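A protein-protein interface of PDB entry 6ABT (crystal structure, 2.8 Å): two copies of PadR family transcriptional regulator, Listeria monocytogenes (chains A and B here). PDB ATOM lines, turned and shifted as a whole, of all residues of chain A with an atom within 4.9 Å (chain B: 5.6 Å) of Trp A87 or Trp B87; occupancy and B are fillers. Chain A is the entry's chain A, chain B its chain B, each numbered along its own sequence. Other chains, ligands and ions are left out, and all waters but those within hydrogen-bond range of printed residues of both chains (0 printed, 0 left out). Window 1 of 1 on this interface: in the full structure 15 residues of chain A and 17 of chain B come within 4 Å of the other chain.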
ATOM      1  N   SER A   5     -28.115 -13.868  14.663  1.00  0.00           N
ATOM      2  CA  SER A   5     -28.008 -12.441  14.993  1.00  0.00           C
ATOM      3  C   SER A   5     -29.364 -11.850  15.381  1.00  0.00           C
ATOM      4  O   SER A   5     -29.439 -10.869  16.113  1.00  0.00           O
ATOM      5  CB  SER A   5     -27.376 -11.661  13.834  1.00  0.00           C
ATOM      6  OG  SER A   5     -26.079 -12.148  13.554  1.00  0.00           O
ATOM      7  N   PHE A  83     -22.504  -8.622  22.031  1.00  0.00           N
ATOM      8  CA  PHE A  83     -22.900  -8.934  20.643  1.00  0.00           C
ATOM      9  C   PHE A  83     -22.210  -8.010  19.610  1.00  0.00           C
ATOM     10  O   PHE A  83     -21.611  -8.516  18.667  1.00  0.00           O
ATOM     11  CB  PHE A  83     -24.460  -8.946  20.544  1.00  0.00           C
ATOM     12  CG  PHE A  83     -25.030  -8.934  19.139  1.00  0.00           C
ATOM     13  CD1 PHE A  83     -25.522  -7.739  18.582  1.00  0.00           C
ATOM     14  CD2 PHE A  83     -25.131 -10.096  18.397  1.00  0.00           C
ATOM     15  CE1 PHE A  83     -26.075  -7.703  17.298  1.00  0.00           C
ATOM     16  CE2 PHE A  83     -25.678 -10.076  17.119  1.00  0.00           C
ATOM     17  CZ  PHE A  83     -26.154  -8.878  16.566  1.00  0.00           C
ATOM     18  N   TRP A  84     -22.274  -6.684  19.792  1.00  0.00           N
ATOM     19  CA  TRP A  84     -21.576  -5.758  18.868  1.00  0.00           C
ATOM     20  C   TRP A  84     -20.071  -6.002  18.782  1.00  0.00           C
ATOM     21  O   TRP A  84     -19.536  -6.093  17.680  1.00  0.00           O
ATOM     22  CB  TRP A  84     -21.899  -4.277  19.115  1.00  0.00           C
ATOM     23  CG  TRP A  84     -23.314  -3.933  18.711  1.00  0.00           C
ATOM     24  CD1 TRP A  84     -24.272  -3.337  19.495  1.00  0.00           C
ATOM     25  CD2 TRP A  84     -23.958  -4.209  17.439  1.00  0.00           C
ATOM     26  NE1 TRP A  84     -25.453  -3.223  18.795  1.00  0.00           N
ATOM     27  CE2 TRP A  84     -25.294  -3.749  17.539  1.00  0.00           C
ATOM     28  CE3 TRP A  84     -23.537  -4.810  16.237  1.00  0.00           C
ATOM     29  CZ2 TRP A  84     -26.223  -3.858  16.472  1.00  0.00           C
ATOM     30  CZ3 TRP A  84     -24.457  -4.918  15.169  1.00  0.00           C
ATOM     31  CH2 TRP A  84     -25.790  -4.445  15.301  1.00  0.00           C
ATOM     32  N   LYS A  85     -19.425  -6.152  19.947  1.00  0.00           N
ATOM     33  CA  LYS A  85     -17.995  -6.505  20.076  1.00  0.00           C
ATOM     34  C   LYS A  85     -17.663  -7.765  19.284  1.00  0.00           C
ATOM     35  O   LYS A  85     -16.626  -7.828  18.600  1.00  0.00           O
ATOM     36  CB  LYS A  85     -17.612  -6.706  21.548  1.00  0.00           C
ATOM     37  N   ARG A  86     -18.563  -8.749  19.369  1.00  0.00           N
ATOM     38  CA  ARG A  86     -18.479  -9.971  18.574  1.00  0.00           C
ATOM     39  C   ARG A  86     -18.616  -9.734  17.062  1.00  0.00           C
ATOM     40  O   ARG A  86     -17.821 -10.283  16.291  1.00  0.00           O
ATOM     41  CB  ARG A  86     -19.483 -11.006  19.080  1.00  0.00           C
ATOM     42  CG  ARG A  86     -18.883 -12.072  19.982  1.00  0.00           C
ATOM     43  CD  ARG A  86     -18.164 -11.519  21.217  1.00  0.00           C
ATOM     44  NE  ARG A  86     -17.409 -12.542  21.959  1.00  0.00           N
ATOM     45  CZ  ARG A  86     -17.936 -13.389  22.844  1.00  0.00           C
ATOM     46  NH1 ARG A  86     -19.243 -13.377  23.116  1.00  0.00           N
ATOM     47  NH2 ARG A  86     -17.152 -14.258  23.461  1.00  0.00           N
ATOM     48  N   TRP A  87     -19.592  -8.916  16.635  1.00  0.00           N
ATOM     49  CA  TRP A  87     -19.675  -8.558  15.212  1.00  0.00           C
ATOM     50  C   TRP A  87     -18.403  -7.867  14.731  1.00  0.00           C
ATOM     51  O   TRP A  87     -17.819  -8.272  13.737  1.00  0.00           O
ATOM     52  CB  TRP A  87     -20.934  -7.774  14.858  1.00  0.00           C
ATOM     53  CG  TRP A  87     -22.003  -8.687  14.307  1.00  0.00           C
ATOM     54  CD1 TRP A  87     -23.137  -9.139  14.970  1.00  0.00           C
ATOM     55  CD2 TRP A  87     -22.041  -9.299  13.012  1.00  0.00           C
ATOM     56  NE1 TRP A  87     -23.869  -9.975  14.158  1.00  0.00           N
ATOM     57  CE2 TRP A  87     -23.224 -10.096  12.954  1.00  0.00           C
ATOM     58  CE3 TRP A  87     -21.201  -9.257  11.894  1.00  0.00           C
ATOM     59  CZ2 TRP A  87     -23.580 -10.836  11.813  1.00  0.00           C
ATOM     60  CZ3 TRP A  87     -21.551  -9.998  10.754  1.00  0.00           C
ATOM     61  CH2 TRP A  87     -22.732 -10.778  10.727  1.00  0.00           C
ATOM     62  N   ASP A  88     -17.976  -6.856  15.480  1.00  0.00           N
ATOM     63  CA  ASP A  88     -16.706  -6.178  15.261  1.00  0.00           C
ATOM     64  C   ASP A  88     -15.542  -7.175  15.102  1.00  0.00           C
ATOM     65  O   ASP A  88     -14.792  -7.109  14.121  1.00  0.00           O
ATOM     66  CB  ASP A  88     -16.436  -5.191  16.402  1.00  0.00           C
ATOM     67  CG  ASP A  88     -17.417  -4.012  16.419  1.00  0.00           C
ATOM     68  OD1 ASP A  88     -17.892  -3.602  15.335  1.00  0.00           O
ATOM     69  OD2 ASP A  88     -17.716  -3.488  17.521  1.00  0.00           O
ATOM     70  N   PHE A  89     -15.439  -8.122  16.037  1.00  0.00           N
ATOM     71  CA  PHE A  89     -14.431  -9.171  15.960  1.00  0.00           C
ATOM     72  C   PHE A  89     -14.476  -9.951  14.664  1.00  0.00           C
ATOM     73  O   PHE A  89     -13.464 -10.130  14.001  1.00  0.00           O
ATOM     74  CB  PHE A  89     -14.519 -10.167  17.118  1.00  0.00           C
ATOM     75  CG  PHE A  89     -13.557 -11.310  16.962  1.00  0.00           C
ATOM     76  CD1 PHE A  89     -12.171 -11.094  17.076  1.00  0.00           C
ATOM     77  CD2 PHE A  89     -14.016 -12.583  16.613  1.00  0.00           C
ATOM     78  CE1 PHE A  89     -11.274 -12.134  16.879  1.00  0.00           C
ATOM     79  CE2 PHE A  89     -13.119 -13.631  16.417  1.00  0.00           C
ATOM     80  CZ  PHE A  89     -11.750 -13.403  16.552  1.00  0.00           C
ATOM     81  N   ILE A  90     -15.656 -10.432  14.322  1.00  0.00           N
ATOM     82  CA  ILE A  90     -15.809 -11.299  13.163  1.00  0.00           C
ATOM     83  C   ILE A  90     -15.796 -10.560  11.827  1.00  0.00           C
ATOM     84  O   ILE A  90     -15.323 -11.104  10.849  1.00  0.00           O
ATOM     85  CB  ILE A  90     -16.999 -12.292  13.336  1.00  0.00           C
ATOM     86  CG1 ILE A  90     -16.556 -13.729  13.006  1.00  0.00           C
ATOM     87  CG2 ILE A  90     -18.251 -11.862  12.576  1.00  0.00           C
ATOM     88  CD1 ILE A  90     -15.485 -14.291  13.917  1.00  0.00           C
ATOM     89  N   GLN A  91     -16.294  -9.324  11.802  1.00  0.00           N
ATOM     90  CA  GLN A  91     -16.220  -8.464  10.622  1.00  0.00           C
ATOM     91  C   GLN A  91     -14.748  -8.160  10.319  1.00  0.00           C
ATOM     92  O   GLN A  91     -14.294  -8.312   9.185  1.00  0.00           O
ATOM     93  CB  GLN A  91     -17.039  -7.182  10.835  1.00  0.00           C
ATOM     94  CG  GLN A  91     -18.547  -7.425  10.820  1.00  0.00           C
ATOM     95  CD  GLN A  91     -19.423  -6.193  11.151  1.00  0.00           C
ATOM     96  OE1 GLN A  91     -20.197  -6.202  12.125  1.00  0.00           O
ATOM     97  NE2 GLN A  91     -19.322  -5.147  10.322  1.00  0.00           N
ATOM     98  N   GLY A  92     -14.008  -7.784  11.360  1.00  0.00           N
ATOM     99  CA  GLY A  92     -12.596  -7.447  11.241  1.00  0.00           C
ATOM    100  C   GLY A  92     -11.721  -8.526  10.646  1.00  0.00           C
ATOM    101  O   GLY A  92     -10.904  -8.242   9.763  1.00  0.00           O
ATOM    102  N   ILE A  94     -12.762 -11.412   8.964  1.00  0.00           N
ATOM    103  CA  ILE A  94     -13.283 -11.694   7.622  1.00  0.00           C
ATOM    104  C   ILE A  94     -12.715 -10.706   6.613  1.00  0.00           C
ATOM    105  O   ILE A  94     -12.215 -11.110   5.556  1.00  0.00           O
ATOM    106  CB  ILE A  94     -14.840 -11.667   7.594  1.00  0.00           C
ATOM    107  CG1 ILE A  94     -15.451 -12.853   8.374  1.00  0.00           C
ATOM    108  CG2 ILE A  94     -15.399 -11.603   6.175  1.00  0.00           C
ATOM    109  CD1 ILE A  94     -14.745 -14.194   8.271  1.00  0.00           C
ATOM    110  N   SER B   5     -19.666 -19.326   5.688  1.00  0.00           N
ATOM    111  CA  SER B   5     -18.505 -18.724   5.036  1.00  0.00           C
ATOM    112  C   SER B   5     -17.396 -19.709   4.639  1.00  0.00           C
ATOM    113  O   SER B   5     -16.652 -19.442   3.701  1.00  0.00           O
ATOM    114  CB  SER B   5     -17.925 -17.601   5.904  1.00  0.00           C
ATOM    115  OG  SER B   5     -18.735 -16.444   5.843  1.00  0.00           O
ATOM    116  N   ILE B  82     -19.123 -13.632  -6.312  1.00  0.00           N
ATOM    117  CA  ILE B  82     -20.482 -13.476  -5.754  1.00  0.00           C
ATOM    118  C   ILE B  82     -20.477 -13.515  -4.227  1.00  0.00           C
ATOM    119  O   ILE B  82     -21.035 -12.632  -3.591  1.00  0.00           O
ATOM    120  CB  ILE B  82     -21.518 -14.481  -6.321  1.00  0.00           C
ATOM    121  CG1 ILE B  82     -21.572 -14.415  -7.846  1.00  0.00           C
ATOM    122  CG2 ILE B  82     -22.904 -14.159  -5.792  1.00  0.00           C
ATOM    123  CD1 ILE B  82     -21.673 -15.782  -8.503  1.00  0.00           C
ATOM    124  N   PHE B  83     -19.844 -14.535  -3.662  1.00  0.00           N
ATOM    125  CA  PHE B  83     -19.676 -14.700  -2.213  1.00  0.00           C
ATOM    126  C   PHE B  83     -19.283 -13.394  -1.501  1.00  0.00           C
ATOM    127  O   PHE B  83     -19.922 -13.022  -0.518  1.00  0.00           O
ATOM    128  CB  PHE B  83     -18.658 -15.840  -1.947  1.00  0.00           C
ATOM    129  CG  PHE B  83     -18.140 -15.909  -0.529  1.00  0.00           C
ATOM    130  CD1 PHE B  83     -18.935 -16.391   0.503  1.00  0.00           C
ATOM    131  CD2 PHE B  83     -16.837 -15.510  -0.235  1.00  0.00           C
ATOM    132  CE1 PHE B  83     -18.448 -16.464   1.804  1.00  0.00           C
ATOM    133  CE2 PHE B  83     -16.332 -15.584   1.065  1.00  0.00           C
ATOM    134  CZ  PHE B  83     -17.139 -16.067   2.084  1.00  0.00           C
ATOM    135  N   TRP B  84     -18.247 -12.713  -2.003  1.00  0.00           N
ATOM    136  CA  TRP B  84     -17.811 -11.434  -1.427  1.00  0.00           C
ATOM    137  C   TRP B  84     -18.847 -10.313  -1.507  1.00  0.00           C
ATOM    138  O   TRP B  84     -19.068  -9.616  -0.518  1.00  0.00           O
ATOM    139  CB  TRP B  84     -16.450 -10.986  -1.974  1.00  0.00           C
ATOM    140  CG  TRP B  84     -15.307 -11.784  -1.408  1.00  0.00           C
ATOM    141  CD1 TRP B  84     -14.326 -12.436  -2.119  1.00  0.00           C
ATOM    142  CD2 TRP B  84     -15.031 -12.061  -0.009  1.00  0.00           C
ATOM    143  NE1 TRP B  84     -13.466 -13.091  -1.254  1.00  0.00           N
ATOM    144  CE2 TRP B  84     -13.868 -12.874   0.037  1.00  0.00           C
ATOM    145  CE3 TRP B  84     -15.653 -11.701   1.200  1.00  0.00           C
ATOM    146  CZ2 TRP B  84     -13.305 -13.316   1.237  1.00  0.00           C
ATOM    147  CZ3 TRP B  84     -15.098 -12.154   2.400  1.00  0.00           C
ATOM    148  CH2 TRP B  84     -13.926 -12.947   2.406  1.00  0.00           C
ATOM    149  N   LYS B  85     -19.480 -10.170  -2.675  1.00  0.00           N
ATOM    150  CA  LYS B  85     -20.626  -9.255  -2.877  1.00  0.00           C
ATOM    151  C   LYS B  85     -21.779  -9.568  -1.916  1.00  0.00           C
ATOM    152  O   LYS B  85     -22.432  -8.649  -1.409  1.00  0.00           O
ATOM    153  CB  LYS B  85     -21.115  -9.288  -4.332  1.00  0.00           C
ATOM    154  N   ARG B  86     -22.007 -10.856  -1.654  1.00  0.00           N
ATOM    155  CA  ARG B  86     -22.915 -11.291  -0.588  1.00  0.00           C
ATOM    156  C   ARG B  86     -22.440 -10.839   0.795  1.00  0.00           C
ATOM    157  O   ARG B  86     -23.248 -10.383   1.593  1.00  0.00           O
ATOM    158  CB  ARG B  86     -23.137 -12.811  -0.622  1.00  0.00           C
ATOM    159  N   TRP B  87     -21.136 -10.929   1.068  1.00  0.00           N
ATOM    160  CA  TRP B  87     -20.616 -10.480   2.354  1.00  0.00           C
ATOM    161  C   TRP B  87     -20.755  -8.995   2.563  1.00  0.00           C
ATOM    162  O   TRP B  87     -21.275  -8.568   3.593  1.00  0.00           O
ATOM    163  CB  TRP B  87     -19.176 -10.927   2.594  1.00  0.00           C
ATOM    164  CG  TRP B  87     -19.123 -12.005   3.620  1.00  0.00           C
ATOM    165  CD1 TRP B  87     -18.803 -13.334   3.408  1.00  0.00           C
ATOM    166  CD2 TRP B  87     -19.448 -11.893   5.018  1.00  0.00           C
ATOM    167  NE1 TRP B  87     -18.903 -14.042   4.589  1.00  0.00           N
ATOM    168  CE2 TRP B  87     -19.293 -13.187   5.593  1.00  0.00           C
ATOM    169  CE3 TRP B  87     -19.862 -10.833   5.845  1.00  0.00           C
ATOM    170  CZ2 TRP B  87     -19.519 -13.440   6.966  1.00  0.00           C
ATOM    171  CZ3 TRP B  87     -20.097 -11.083   7.213  1.00  0.00           C
ATOM    172  CH2 TRP B  87     -19.918 -12.377   7.755  1.00  0.00           C
ATOM    173  N   ASP B  88     -20.283  -8.235   1.576  1.00  0.00           N
ATOM    174  CA  ASP B  88     -20.365  -6.778   1.537  1.00  0.00           C
ATOM    175  C   ASP B  88     -21.781  -6.289   1.856  1.00  0.00           C
ATOM    176  O   ASP B  88     -21.966  -5.399   2.696  1.00  0.00           O
ATOM    177  CB  ASP B  88     -19.936  -6.264   0.147  1.00  0.00           C
ATOM    178  CG  ASP B  88     -18.430  -6.452  -0.124  1.00  0.00           C
ATOM    179  OD1 ASP B  88     -17.626  -6.242   0.813  1.00  0.00           O
ATOM    180  OD2 ASP B  88     -18.048  -6.807  -1.275  1.00  0.00           O
ATOM    181  N   PHE B  89     -22.762  -6.908   1.193  1.00  0.00           N
ATOM    182  CA  PHE B  89     -24.167  -6.661   1.413  1.00  0.00           C
ATOM    183  C   PHE B  89     -24.599  -6.760   2.871  1.00  0.00           C
ATOM    184  O   PHE B  89     -25.190  -5.831   3.423  1.00  0.00           O
ATOM    185  CB  PHE B  89     -25.001  -7.633   0.573  1.00  0.00           C
ATOM    186  CG  PHE B  89     -26.466  -7.554   0.867  1.00  0.00           C
ATOM    187  CD1 PHE B  89     -27.210  -6.419   0.488  1.00  0.00           C
ATOM    188  CD2 PHE B  89     -27.100  -8.585   1.566  1.00  0.00           C
ATOM    189  CE1 PHE B  89     -28.564  -6.323   0.789  1.00  0.00           C
ATOM    190  CE2 PHE B  89     -28.457  -8.497   1.869  1.00  0.00           C
ATOM    191  CZ  PHE B  89     -29.193  -7.365   1.477  1.00  0.00           C
ATOM    192  N   ILE B  90     -24.318  -7.905   3.472  1.00  0.00           N
ATOM    193  CA  ILE B  90     -24.753  -8.200   4.833  1.00  0.00           C
ATOM    194  C   ILE B  90     -24.050  -7.350   5.904  1.00  0.00           C
ATOM    195  O   ILE B  90     -24.721  -6.829   6.794  1.00  0.00           O
ATOM    196  CB  ILE B  90     -24.751  -9.741   5.126  1.00  0.00           C
ATOM    197  CG1 ILE B  90     -26.158 -10.196   5.568  1.00  0.00           C
ATOM    198  CG2 ILE B  90     -23.634 -10.193   6.081  1.00  0.00           C
ATOM    199  CD1 ILE B  90     -26.999 -10.766   4.450  1.00  0.00           C
ATOM    200  N   GLN B  91     -22.734  -7.174   5.785  1.00  0.00           N
ATOM    201  CA  GLN B  91     -21.987  -6.248   6.643  1.00  0.00           C
ATOM    202  C   GLN B  91     -22.558  -4.828   6.569  1.00  0.00           C
ATOM    203  O   GLN B  91     -22.777  -4.184   7.604  1.00  0.00           O
ATOM    204  CB  GLN B  91     -20.502  -6.235   6.279  1.00  0.00           C
ATOM    205  CG  GLN B  91     -19.756  -7.462   6.759  1.00  0.00           C
ATOM    206  CD  GLN B  91     -18.260  -7.404   6.479  1.00  0.00           C
ATOM    207  OE1 GLN B  91     -17.625  -6.368   6.692  1.00  0.00           O
ATOM    208  NE2 GLN B  91     -17.686  -8.523   6.014  1.00  0.00           N
ATOM    209  N   GLY B  92     -22.810  -4.373   5.338  1.00  0.00           N
ATOM    210  CA  GLY B  92     -23.368  -3.069   5.072  1.00  0.00           C
ATOM    211  C   GLY B  92     -24.696  -2.865   5.763  1.00  0.00           C
ATOM    212  O   GLY B  92     -24.921  -1.804   6.347  1.00  0.00           O
ATOM    213  N   ILE B  94     -25.998  -4.634   8.434  1.00  0.00           N
ATOM    214  CA  ILE B  94     -25.721  -4.669   9.863  1.00  0.00           C
ATOM    215  C   ILE B  94     -25.161  -3.321  10.308  1.00  0.00           C
ATOM    216  O   ILE B  94     -25.535  -2.811  11.365  1.00  0.00           O
ATOM    217  CB  ILE B  94     -24.747  -5.830  10.182  1.00  0.00           C
ATOM    218  CG1 ILE B  94     -25.477  -7.160  10.026  1.00  0.00           C
ATOM    219  CG2 ILE B  94     -24.125  -5.718  11.573  1.00  0.00           C
ATOM    220  CD1 ILE B  94     -24.589  -8.273   9.518  1.00  0.00           C
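Lys A85 touches none of the printed residues of chain B. Of the printed residues of chain B, Trp A87 touches Trp B87 (3.98 Å) and Ile B94 (3.3 Å). Of the printed residues of chain B, Gln A91 touches Ile B94. Printed residues of chain B within 4 Å of Ile A94: Trp B84 (3.8 Å) and Gln B91 (3.8 Å). Of chain A, only Trp A87 (3.98 Å) comes within 4 Å of Trp B87. Printed residues of chain A within 4 Å of Gln B91: Ile A94 (3.8 Å). Gly B92 touches none of the printed residues of chain A. The nearest printed residue of chain B that does not touch Gln A91 is Gln B91 (4.2 Å).
Hydrophobic or aromatic side chains of chain B that line the printed part of chain A: Trp B84, Trp B87 and Ile B94. Hydrophobic or aromatic side chains of chain A that line the printed part of chain B: Trp A84, Trp A87 and Ile A94. Among the printed residues, no Asp or Glu carboxylate lies within 4 Å of a Lys or Arg side-chain nitrogen of the other chain.
Trp A84 touches Ile B94, and with the chains exchanged Ile A94 touches Trp B84. Trp A87 touches its own counterpart, Trp B87. Trp A87 touches Ile B94, but with the chains exchanged Ile A94 does not touch Trp B87 (4.2 Å). Gln A91 touches Ile B94, and with the chains exchanged Ile A94 touches Gln B91. Of the 6 pairs that touch across the chains among the printed residues, 5 have their exchanged pair printed and touching as well.
OG of Ser A5 sits at hydrogen-bond distance from NE1 of Trp A87 (3.2 Å). The side-chain hydroxyl (OG) of Ser B5 is in hydrogen-bond range of the indole nitrogen (NE1) of Trp B87 (2.7 Å).
Among the printed residues, pairs that only touch across the chains: Trp A87 with Ile B94 (3.3 Å), Trp A84 with Ile B94 (3.7 Å), Ile A94 with Trp B84 (3.8 Å), Ile A94 with Gln B91 (3.8 Å), Trp A87 with Trp B87 (3.98 Å) and Gln A91 with Ile B94 (3.996 Å).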
